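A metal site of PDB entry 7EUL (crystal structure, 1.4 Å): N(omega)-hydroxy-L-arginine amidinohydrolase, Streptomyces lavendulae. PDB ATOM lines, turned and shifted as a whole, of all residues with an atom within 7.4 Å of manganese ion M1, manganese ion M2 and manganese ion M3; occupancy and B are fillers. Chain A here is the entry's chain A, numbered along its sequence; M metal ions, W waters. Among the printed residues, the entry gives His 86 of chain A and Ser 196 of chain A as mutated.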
ATOM      1  N   MET A  18      11.731  16.087  11.572  1.00  0.00           N
ATOM      2  CA  MET A  18      10.700  15.195  12.072  1.00  0.00           C
ATOM      3  C   MET A  18       9.293  15.738  11.819  1.00  0.00           C
ATOM      4  O   MET A  18       8.376  14.933  11.624  1.00  0.00           O
ATOM      5  CB  MET A  18      10.934  14.812  13.531  1.00  0.00           C
ATOM      6  CG  MET A  18      11.790  13.556  13.678  1.00  0.00           C
ATOM      7  SD  MET A  18      12.230  13.248  15.394  1.00  0.00           S
ATOM      8  CE  MET A  18      12.696  14.934  15.825  1.00  0.00           C
ATOM      9  N   THR A  85       7.343  13.853  17.001  1.00  0.00           N
ATOM     10  CA  THR A  85       8.186  13.251  18.027  1.00  0.00           C
ATOM     11  C   THR A  85       7.362  12.354  18.943  1.00  0.00           C
ATOM     12  O   THR A  85       6.149  12.508  19.076  1.00  0.00           O
ATOM     13  CB  THR A  85       8.884  14.304  18.902  1.00  0.00           C
ATOM     14  OG1 THR A  85       7.906  15.020  19.671  1.00  0.00           O
ATOM     15  CG2 THR A  85       9.687  15.289  18.056  1.00  0.00           C
ATOM     16  N   HIS A  86       8.067  11.425  19.593  1.00  0.00           N
ATOM     17  CA  HIS A  86       7.441  10.523  20.559  1.00  0.00           C
ATOM     18  C   HIS A  86       6.890  11.277  21.765  1.00  0.00           C
ATOM     19  O   HIS A  86       6.011  10.755  22.458  1.00  0.00           O
ATOM     20  CB  HIS A  86       8.465   9.509  21.038  1.00  0.00           C
ATOM     21  CG  HIS A  86       7.891   8.154  21.297  1.00  0.00           C
ATOM     22  ND1 HIS A  86       8.688   7.065  21.510  1.00  0.00           N
ATOM     23  CD2 HIS A  86       6.608   7.733  21.362  1.00  0.00           C
ATOM     24  CE1 HIS A  86       7.916   5.988  21.652  1.00  0.00           C
ATOM     25  NE2 HIS A  86       6.656   6.375  21.611  1.00  0.00           N
ATOM     26  N   SER A  87       7.408  12.480  22.035  1.00  0.00           N
ATOM     27  CA  SER A  87       6.941  13.264  23.182  1.00  0.00           C
ATOM     28  C   SER A  87       5.467  13.658  23.068  1.00  0.00           C
ATOM     29  O   SER A  87       4.855  13.953  24.090  1.00  0.00           O
ATOM     30  CB  SER A  87       7.820  14.495  23.361  1.00  0.00           C
ATOM     31  OG  SER A  87       9.156  14.116  23.723  1.00  0.00           O
ATOM     32  N   TYR A 107       4.825  -0.369  23.712  1.00  0.00           N
ATOM     33  CA  TYR A 107       5.687   0.798  23.509  1.00  0.00           C
ATOM     34  C   TYR A 107       6.928   0.307  22.751  1.00  0.00           C
ATOM     35  O   TYR A 107       7.844  -0.271  23.334  1.00  0.00           O
ATOM     36  CB  TYR A 107       6.010   1.421  24.851  1.00  0.00           C
ATOM     37  CG  TYR A 107       6.544   2.837  24.805  1.00  0.00           C
ATOM     38  CD1 TYR A 107       7.909   3.076  24.641  1.00  0.00           C
ATOM     39  CD2 TYR A 107       5.701   3.930  24.974  1.00  0.00           C
ATOM     40  CE1 TYR A 107       8.414   4.388  24.603  1.00  0.00           C
ATOM     41  CE2 TYR A 107       6.201   5.229  24.939  1.00  0.00           C
ATOM     42  CZ  TYR A 107       7.552   5.456  24.766  1.00  0.00           C
ATOM     43  OH  TYR A 107       8.048   6.742  24.735  1.00  0.00           O
ATOM     44  N   ILE A 108       6.914   0.481  21.439  1.00  0.00           N
ATOM     45  CA  ILE A 108       7.872  -0.170  20.555  1.00  0.00           C
ATOM     46  C   ILE A 108       8.946   0.855  20.248  1.00  0.00           C
ATOM     47  O   ILE A 108       8.687   1.841  19.543  1.00  0.00           O
ATOM     48  CB  ILE A 108       7.171  -0.698  19.296  1.00  0.00           C
ATOM     49  CG1 ILE A 108       5.972  -1.587  19.697  1.00  0.00           C
ATOM     50  CG2 ILE A 108       8.169  -1.481  18.421  1.00  0.00           C
ATOM     51  CD1 ILE A 108       5.278  -2.278  18.522  1.00  0.00           C
ATOM     52  N   ASP A 109      10.146   0.636  20.782  1.00  0.00           N
ATOM     53  CA  ASP A 109      11.113   1.709  20.909  1.00  0.00           C
ATOM     54  C   ASP A 109      12.494   1.109  21.116  1.00  0.00           C
ATOM     55  O   ASP A 109      12.633   0.119  21.829  1.00  0.00           O
ATOM     56  CB  ASP A 109      10.743   2.566  22.129  1.00  0.00           C
ATOM     57  CG  ASP A 109      11.395   3.927  22.120  1.00  0.00           C
ATOM     58  OD1 ASP A 109      12.617   4.033  22.260  1.00  0.00           O
ATOM     59  OD2 ASP A 109      10.672   4.906  21.928  1.00  0.00           O
ATOM     60  N   GLY A 110      13.520   1.735  20.540  1.00  0.00           N
ATOM     61  CA  GLY A 110      14.877   1.276  20.770  1.00  0.00           C
ATOM     62  C   GLY A 110      15.424   1.600  22.149  1.00  0.00           C
ATOM     63  O   GLY A 110      16.403   0.991  22.581  1.00  0.00           O
ATOM     64  N   HIS A 111      14.791   2.527  22.846  1.00  0.00           N
ATOM     65  CA  HIS A 111      15.157   2.988  24.169  1.00  0.00           C
ATOM     66  C   HIS A 111      14.001   2.666  25.128  1.00  0.00           C
ATOM     67  O   HIS A 111      12.954   2.148  24.715  1.00  0.00           O
ATOM     68  CB  HIS A 111      15.406   4.496  24.130  1.00  0.00           C
ATOM     69  CG  HIS A 111      16.408   4.909  23.094  1.00  0.00           C
ATOM     70  ND1 HIS A 111      16.044   5.315  21.832  1.00  0.00           N
ATOM     71  CD2 HIS A 111      17.755   4.988  23.144  1.00  0.00           C
ATOM     72  CE1 HIS A 111      17.131   5.618  21.129  1.00  0.00           C
ATOM     73  NE2 HIS A 111      18.184   5.425  21.908  1.00  0.00           N
ATOM     74  N   GLY A 112      14.194   2.941  26.401  1.00  0.00           N
ATOM     75  CA  GLY A 112      13.088   2.743  27.312  1.00  0.00           C
ATOM     76  C   GLY A 112      12.233   3.970  27.563  1.00  0.00           C
ATOM     77  O   GLY A 112      11.122   3.838  28.098  1.00  0.00           O
ATOM     78  N   ASP A 113      12.727   5.155  27.181  1.00  0.00           N
ATOM     79  CA  ASP A 113      12.033   6.414  27.440  1.00  0.00           C
ATOM     80  C   ASP A 113      11.508   6.495  28.879  1.00  0.00           C
ATOM     81  O   ASP A 113      10.398   6.964  29.125  1.00  0.00           O
ATOM     82  CB  ASP A 113      10.930   6.667  26.413  1.00  0.00           C
ATOM     83  CG  ASP A 113      11.471   6.806  25.007  1.00  0.00           C
ATOM     84  OD1 ASP A 113      12.713   6.822  24.816  1.00  0.00           O
ATOM     85  OD2 ASP A 113      10.646   6.928  24.088  1.00  0.00           O
ATOM     86  N   TYR A 124      16.602  15.508  27.671  1.00  0.00           N
ATOM     87  CA  TYR A 124      15.754  15.362  26.488  1.00  0.00           C
ATOM     88  C   TYR A 124      14.379  14.813  26.865  1.00  0.00           C
ATOM     89  O   TYR A 124      14.267  13.708  27.404  1.00  0.00           O
ATOM     90  CB  TYR A 124      16.424  14.467  25.444  1.00  0.00           C
ATOM     91  CG  TYR A 124      15.564  14.284  24.216  1.00  0.00           C
ATOM     92  CD1 TYR A 124      14.916  15.374  23.646  1.00  0.00           C
ATOM     93  CD2 TYR A 124      15.377  13.028  23.638  1.00  0.00           C
ATOM     94  CE1 TYR A 124      14.110  15.230  22.537  1.00  0.00           C
ATOM     95  CE2 TYR A 124      14.567  12.871  22.532  1.00  0.00           C
ATOM     96  CZ  TYR A 124      13.947  13.979  21.986  1.00  0.00           C
ATOM     97  OH  TYR A 124      13.127  13.833  20.878  1.00  0.00           O
ATOM     98  N   GLY A 126      12.103  13.522  25.081  1.00  0.00           N
ATOM     99  CA  GLY A 126      11.761  12.266  24.440  1.00  0.00           C
ATOM    100  C   GLY A 126      12.229  11.036  25.194  1.00  0.00           C
ATOM    101  O   GLY A 126      11.707   9.939  24.966  1.00  0.00           O
ATOM    102  N   GLY A 127      13.207  11.196  26.076  1.00  0.00           N
ATOM    103  CA  GLY A 127      13.649  10.109  26.925  1.00  0.00           C
ATOM    104  C   GLY A 127      12.892   9.958  28.215  1.00  0.00           C
ATOM    105  O   GLY A 127      13.290   9.136  29.053  1.00  0.00           O
ATOM    106  N   VAL A 129       9.182   9.958  28.211  1.00  0.00           N
ATOM    107  CA  VAL A 129       7.777   9.870  27.810  1.00  0.00           C
ATOM    108  C   VAL A 129       7.024   8.794  28.591  1.00  0.00           C
ATOM    109  O   VAL A 129       5.931   9.042  29.111  1.00  0.00           O
ATOM    110  CB  VAL A 129       7.696   9.622  26.294  1.00  0.00           C
ATOM    111  CG1 VAL A 129       6.266   9.445  25.873  1.00  0.00           C
ATOM    112  CG2 VAL A 129       8.349  10.755  25.518  1.00  0.00           C
ATOM    113  N   SER A 196       2.371   2.174  20.247  1.00  0.00           N
ATOM    114  CA  SER A 196       3.117   3.427  20.079  1.00  0.00           C
ATOM    115  C   SER A 196       4.510   3.090  19.592  1.00  0.00           C
ATOM    116  O   SER A 196       5.276   2.445  20.323  1.00  0.00           O
ATOM    117  CB  SER A 196       3.200   4.175  21.406  1.00  0.00           C
ATOM    118  OG  SER A 196       3.846   5.432  21.248  1.00  0.00           O
ATOM    119  N   ILE A 197       4.864   3.515  18.375  1.00  0.00           N
ATOM    120  CA  ILE A 197       6.093   3.122  17.709  1.00  0.00           C
ATOM    121  C   ILE A 197       7.005   4.351  17.525  1.00  0.00           C
ATOM    122  O   ILE A 197       6.531   5.390  17.063  1.00  0.00           O
ATOM    123  CB  ILE A 197       5.814   2.510  16.327  1.00  0.00           C
ATOM    124  CG1 ILE A 197       5.106   1.171  16.465  1.00  0.00           C
ATOM    125  CG2 ILE A 197       7.114   2.353  15.532  1.00  0.00           C
ATOM    126  CD1 ILE A 197       4.611   0.617  15.153  1.00  0.00           C
ATOM    127  N   ASP A 198       8.287   4.188  17.847  1.00  0.00           N
ATOM    128  CA  ASP A 198       9.363   5.142  17.544  1.00  0.00           C
ATOM    129  C   ASP A 198      10.268   4.403  16.564  1.00  0.00           C
ATOM    130  O   ASP A 198      10.773   3.319  16.898  1.00  0.00           O
ATOM    131  CB  ASP A 198      10.101   5.434  18.854  1.00  0.00           C
ATOM    132  CG  ASP A 198      11.262   6.405  18.726  1.00  0.00           C
ATOM    133  OD1 ASP A 198      11.912   6.483  17.665  1.00  0.00           O
ATOM    134  OD2 ASP A 198      11.559   7.100  19.715  1.00  0.00           O
ATOM    135  N   TRP A 199      10.462   4.958  15.362  1.00  0.00           N
ATOM    136  CA  TRP A 199      11.230   4.245  14.324  1.00  0.00           C
ATOM    137  C   TRP A 199      12.687   3.975  14.690  1.00  0.00           C
ATOM    138  O   TRP A 199      13.329   3.184  13.991  1.00  0.00           O
ATOM    139  CB  TRP A 199      11.135   4.922  12.951  1.00  0.00           C
ATOM    140  CG  TRP A 199       9.722   5.039  12.451  1.00  0.00           C
ATOM    141  CD1 TRP A 199       9.072   6.190  12.127  1.00  0.00           C
ATOM    142  CD2 TRP A 199       8.776   3.968  12.240  1.00  0.00           C
ATOM    143  NE1 TRP A 199       7.787   5.912  11.721  1.00  0.00           N
ATOM    144  CE2 TRP A 199       7.582   4.564  11.786  1.00  0.00           C
ATOM    145  CE3 TRP A 199       8.834   2.583  12.394  1.00  0.00           C
ATOM    146  CZ2 TRP A 199       6.446   3.818  11.471  1.00  0.00           C
ATOM    147  CZ3 TRP A 199       7.693   1.834  12.091  1.00  0.00           C
ATOM    148  CH2 TRP A 199       6.516   2.462  11.635  1.00  0.00           C
ATOM    149  N   ASP A 200      13.223   4.558  15.774  1.00  0.00           N
ATOM    150  CA  ASP A 200      14.556   4.135  16.205  1.00  0.00           C
ATOM    151  C   ASP A 200      14.590   2.707  16.749  1.00  0.00           C
ATOM    152  O   ASP A 200      15.675   2.192  17.066  1.00  0.00           O
ATOM    153  CB  ASP A 200      15.204   5.146  17.175  1.00  0.00           C
ATOM    154  CG  ASP A 200      14.505   5.239  18.537  1.00  0.00           C
ATOM    155  OD1 ASP A 200      13.922   4.247  19.017  1.00  0.00           O
ATOM    156  OD2 ASP A 200      14.573   6.331  19.142  1.00  0.00           O
ATOM    157  N   VAL A 201      13.430   2.037  16.862  1.00  0.00           N
ATOM    158  CA  VAL A 201      13.417   0.622  17.222  1.00  0.00           C
ATOM    159  C   VAL A 201      14.064  -0.236  16.135  1.00  0.00           C
ATOM    160  O   VAL A 201      14.572  -1.317  16.415  1.00  0.00           O
ATOM    161  CB  VAL A 201      11.990   0.160  17.553  1.00  0.00           C
ATOM    162  CG1 VAL A 201      11.138   0.038  16.270  1.00  0.00           C
ATOM    163  CG2 VAL A 201      12.032  -1.148  18.312  1.00  0.00           C
ATOM    164  N   ALA A 209      15.694   8.001  11.701  1.00  0.00           N
ATOM    165  CA  ALA A 209      15.048   8.546  12.888  1.00  0.00           C
ATOM    166  C   ALA A 209      15.984   9.551  13.547  1.00  0.00           C
ATOM    167  O   ALA A 209      16.827  10.149  12.875  1.00  0.00           O
ATOM    168  CB  ALA A 209      14.632   7.418  13.851  1.00  0.00           C
ATOM    169  N   ASP A 210      15.837   9.768  14.852  1.00  0.00           N
ATOM    170  CA  ASP A 210      16.730  10.688  15.538  1.00  0.00           C
ATOM    171  C   ASP A 210      17.938   9.961  16.115  1.00  0.00           C
ATOM    172  O   ASP A 210      19.066  10.464  16.035  1.00  0.00           O
ATOM    173  CB  ASP A 210      15.965  11.428  16.653  1.00  0.00           C
ATOM    174  CG  ASP A 210      16.709  12.656  17.171  1.00  0.00           C
ATOM    175  OD1 ASP A 210      17.808  12.951  16.677  1.00  0.00           O
ATOM    176  OD2 ASP A 210      16.159  13.320  18.078  1.00  0.00           O
ATOM    177  N   TYR A 211      17.724   8.776  16.672  1.00  0.00           N
ATOM    178  CA  TYR A 211      18.777   8.002  17.280  1.00  0.00           C
ATOM    179  C   TYR A 211      19.020   6.726  16.498  1.00  0.00           C
ATOM    180  O   TYR A 211      18.159   6.226  15.763  1.00  0.00           O
ATOM    181  CB  TYR A 211      18.450   7.689  18.743  1.00  0.00           C
ATOM    182  CG  TYR A 211      18.491   8.932  19.599  1.00  0.00           C
ATOM    183  CD1 TYR A 211      17.412   9.816  19.614  1.00  0.00           C
ATOM    184  CD2 TYR A 211      19.614   9.251  20.349  1.00  0.00           C
ATOM    185  CE1 TYR A 211      17.442  10.970  20.378  1.00  0.00           C
ATOM    186  CE2 TYR A 211      19.653  10.394  21.115  1.00  0.00           C
ATOM    187  CZ  TYR A 211      18.570  11.255  21.123  1.00  0.00           C
ATOM    188  OH  TYR A 211      18.608  12.398  21.890  1.00  0.00           O
ATOM    189  N   VAL A 213      20.396   3.101  17.272  1.00  0.00           N
ATOM    190  CA  VAL A 213      20.748   2.049  18.212  1.00  0.00           C
ATOM    191  C   VAL A 213      21.032   0.775  17.410  1.00  0.00           C
ATOM    192  O   VAL A 213      20.127   0.301  16.707  1.00  0.00           O
ATOM    193  CB  VAL A 213      19.628   1.812  19.227  1.00  0.00           C
ATOM    194  CG1 VAL A 213      20.172   1.112  20.445  1.00  0.00           C
ATOM    195  CG2 VAL A 213      18.972   3.141  19.611  1.00  0.00           C
ATOM    196  N   ALA A 240       5.855   7.563  15.130  1.00  0.00           N
ATOM    197  CA  ALA A 240       6.655   8.739  15.468  1.00  0.00           C
ATOM    198  C   ALA A 240       8.096   8.603  15.017  1.00  0.00           C
ATOM    199  O   ALA A 240       8.675   7.512  15.028  1.00  0.00           O
ATOM    200  CB  ALA A 240       6.666   8.977  16.990  1.00  0.00           C
ATOM    201  N   GLU A 241       8.666   9.750  14.639  1.00  0.00           N
ATOM    202  CA  GLU A 241      10.098   9.983  14.496  1.00  0.00           C
ATOM    203  C   GLU A 241      10.705   9.538  13.176  1.00  0.00           C
ATOM    204  O   GLU A 241      11.814   8.995  13.136  1.00  0.00           O
ATOM    205  CB  GLU A 241      10.881   9.455  15.698  1.00  0.00           C
ATOM    206  CG  GLU A 241      10.247   9.843  17.026  1.00  0.00           C
ATOM    207  CD  GLU A 241      11.229  10.401  18.008  1.00  0.00           C
ATOM    208  OE1 GLU A 241      12.419  10.070  17.911  1.00  0.00           O
ATOM    209  OE2 GLU A 241      10.800  11.170  18.902  1.00  0.00           O
HETATM  210 MN    MN M   1      10.914   7.010  21.910  1.00  0.00          MN
HETATM  211 MN    MN M   2      13.307   8.214  18.557  1.00  0.00          MN
HETATM  212 MN    MN M   3      13.792   5.704  20.908  1.00  0.00          MN
HETATM  213  O   HOH W   1      13.969   9.177  20.627  1.00  0.00           O
HETATM  214  O   HOH W   2      14.714   8.650  17.363  1.00  0.00           O
HETATM  215  O   HOH W   3      13.145   6.818  22.145  1.00  0.00           O
HETATM  216  O   HOH W   4      11.261   9.136  22.314  1.00  0.00           O
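Manganese ion M3 is bound by water W3, the side-chain carboxylate (OD2) of Asp 200, the side-chain carboxylate (OD1) of Asp 200, the side-chain carboxylate (OD1) of Asp 109 and a ring nitrogen (ND1) of His 111. Slightly farther from manganese ion M3 lies OD2 of Asp 198 (2.9 Å).
Within 4 Å of manganese ion M1: His 86, Asp 109, Asp 113 and Asp 198. The nearest printed residue that does not touch manganese ion M1 is Tyr 107 (4.03 Å).
OD1 of Asp 200 lies close to N of Gly 110 (3.0 Å). The side-chain carboxylate (OE2) of Glu 241 is in hydrogen-bond range of the backbone NH (N) of His 86, at 2.8 Å. OH of Tyr 107 sits close to OD2 of Asp 113 (2.7 Å). The backbone NH (N) of Val 129 is in hydrogen-bond range of the backbone carbonyl oxygen (O) of Asp 113, 3.4 Å away. OH of Tyr 107 lies close to NE2 of His 86. NE2 of His 86 lies within hydrogen-bond range of OG of Ser 196. N of Asp 198 is in hydrogen-bond range of O of Ile 108, at 2.9 Å.
Manganese ion M2 is bound by water W2. Manganese ion M2 is bound by OE1 of Glu 241, 2.2 Å away. Manganese ion M2 is bound by the side-chain carboxylate (OD2) of Asp 200 (2.3 Å). Manganese ion M2 is bound by OD2 of Asp 198. Water W1 binds manganese ion M2. OD1 of Asp 198 binds manganese ion M2 (2.4 Å). Manganese ion M2 has six donor atoms within binding distance.
OD2 of Asp 109 is bound to manganese ion M1 (2.1 Å). Manganese ion M1 is bound by water W4, 2.2 Å away. OD2 of Asp 113 is bound to manganese ion M1, at 2.2 Å. Water W3 is bound to manganese ion M1. ND1 of His 86 is bound to manganese ion M1 (2.3 Å). Manganese ion M1 is bound by the side-chain carboxylate (OD2) of Asp 198, at 2.3 Å. Manganese ion M1 has six donor atoms within binding distance.
The nearest printed residue that does not touch manganese ion M2 is Tyr 211 (4.5 Å).
Gly 110 touches manganese ion M3 (N to MN, 3.995 Å). Within 4 Å of manganese ion M3: Asp 109, Gly 110, His 111, Asp 198 and Asp 200. The nearest printed residue that does not touch manganese ion M3 is Asp 113 (4.2 Å).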
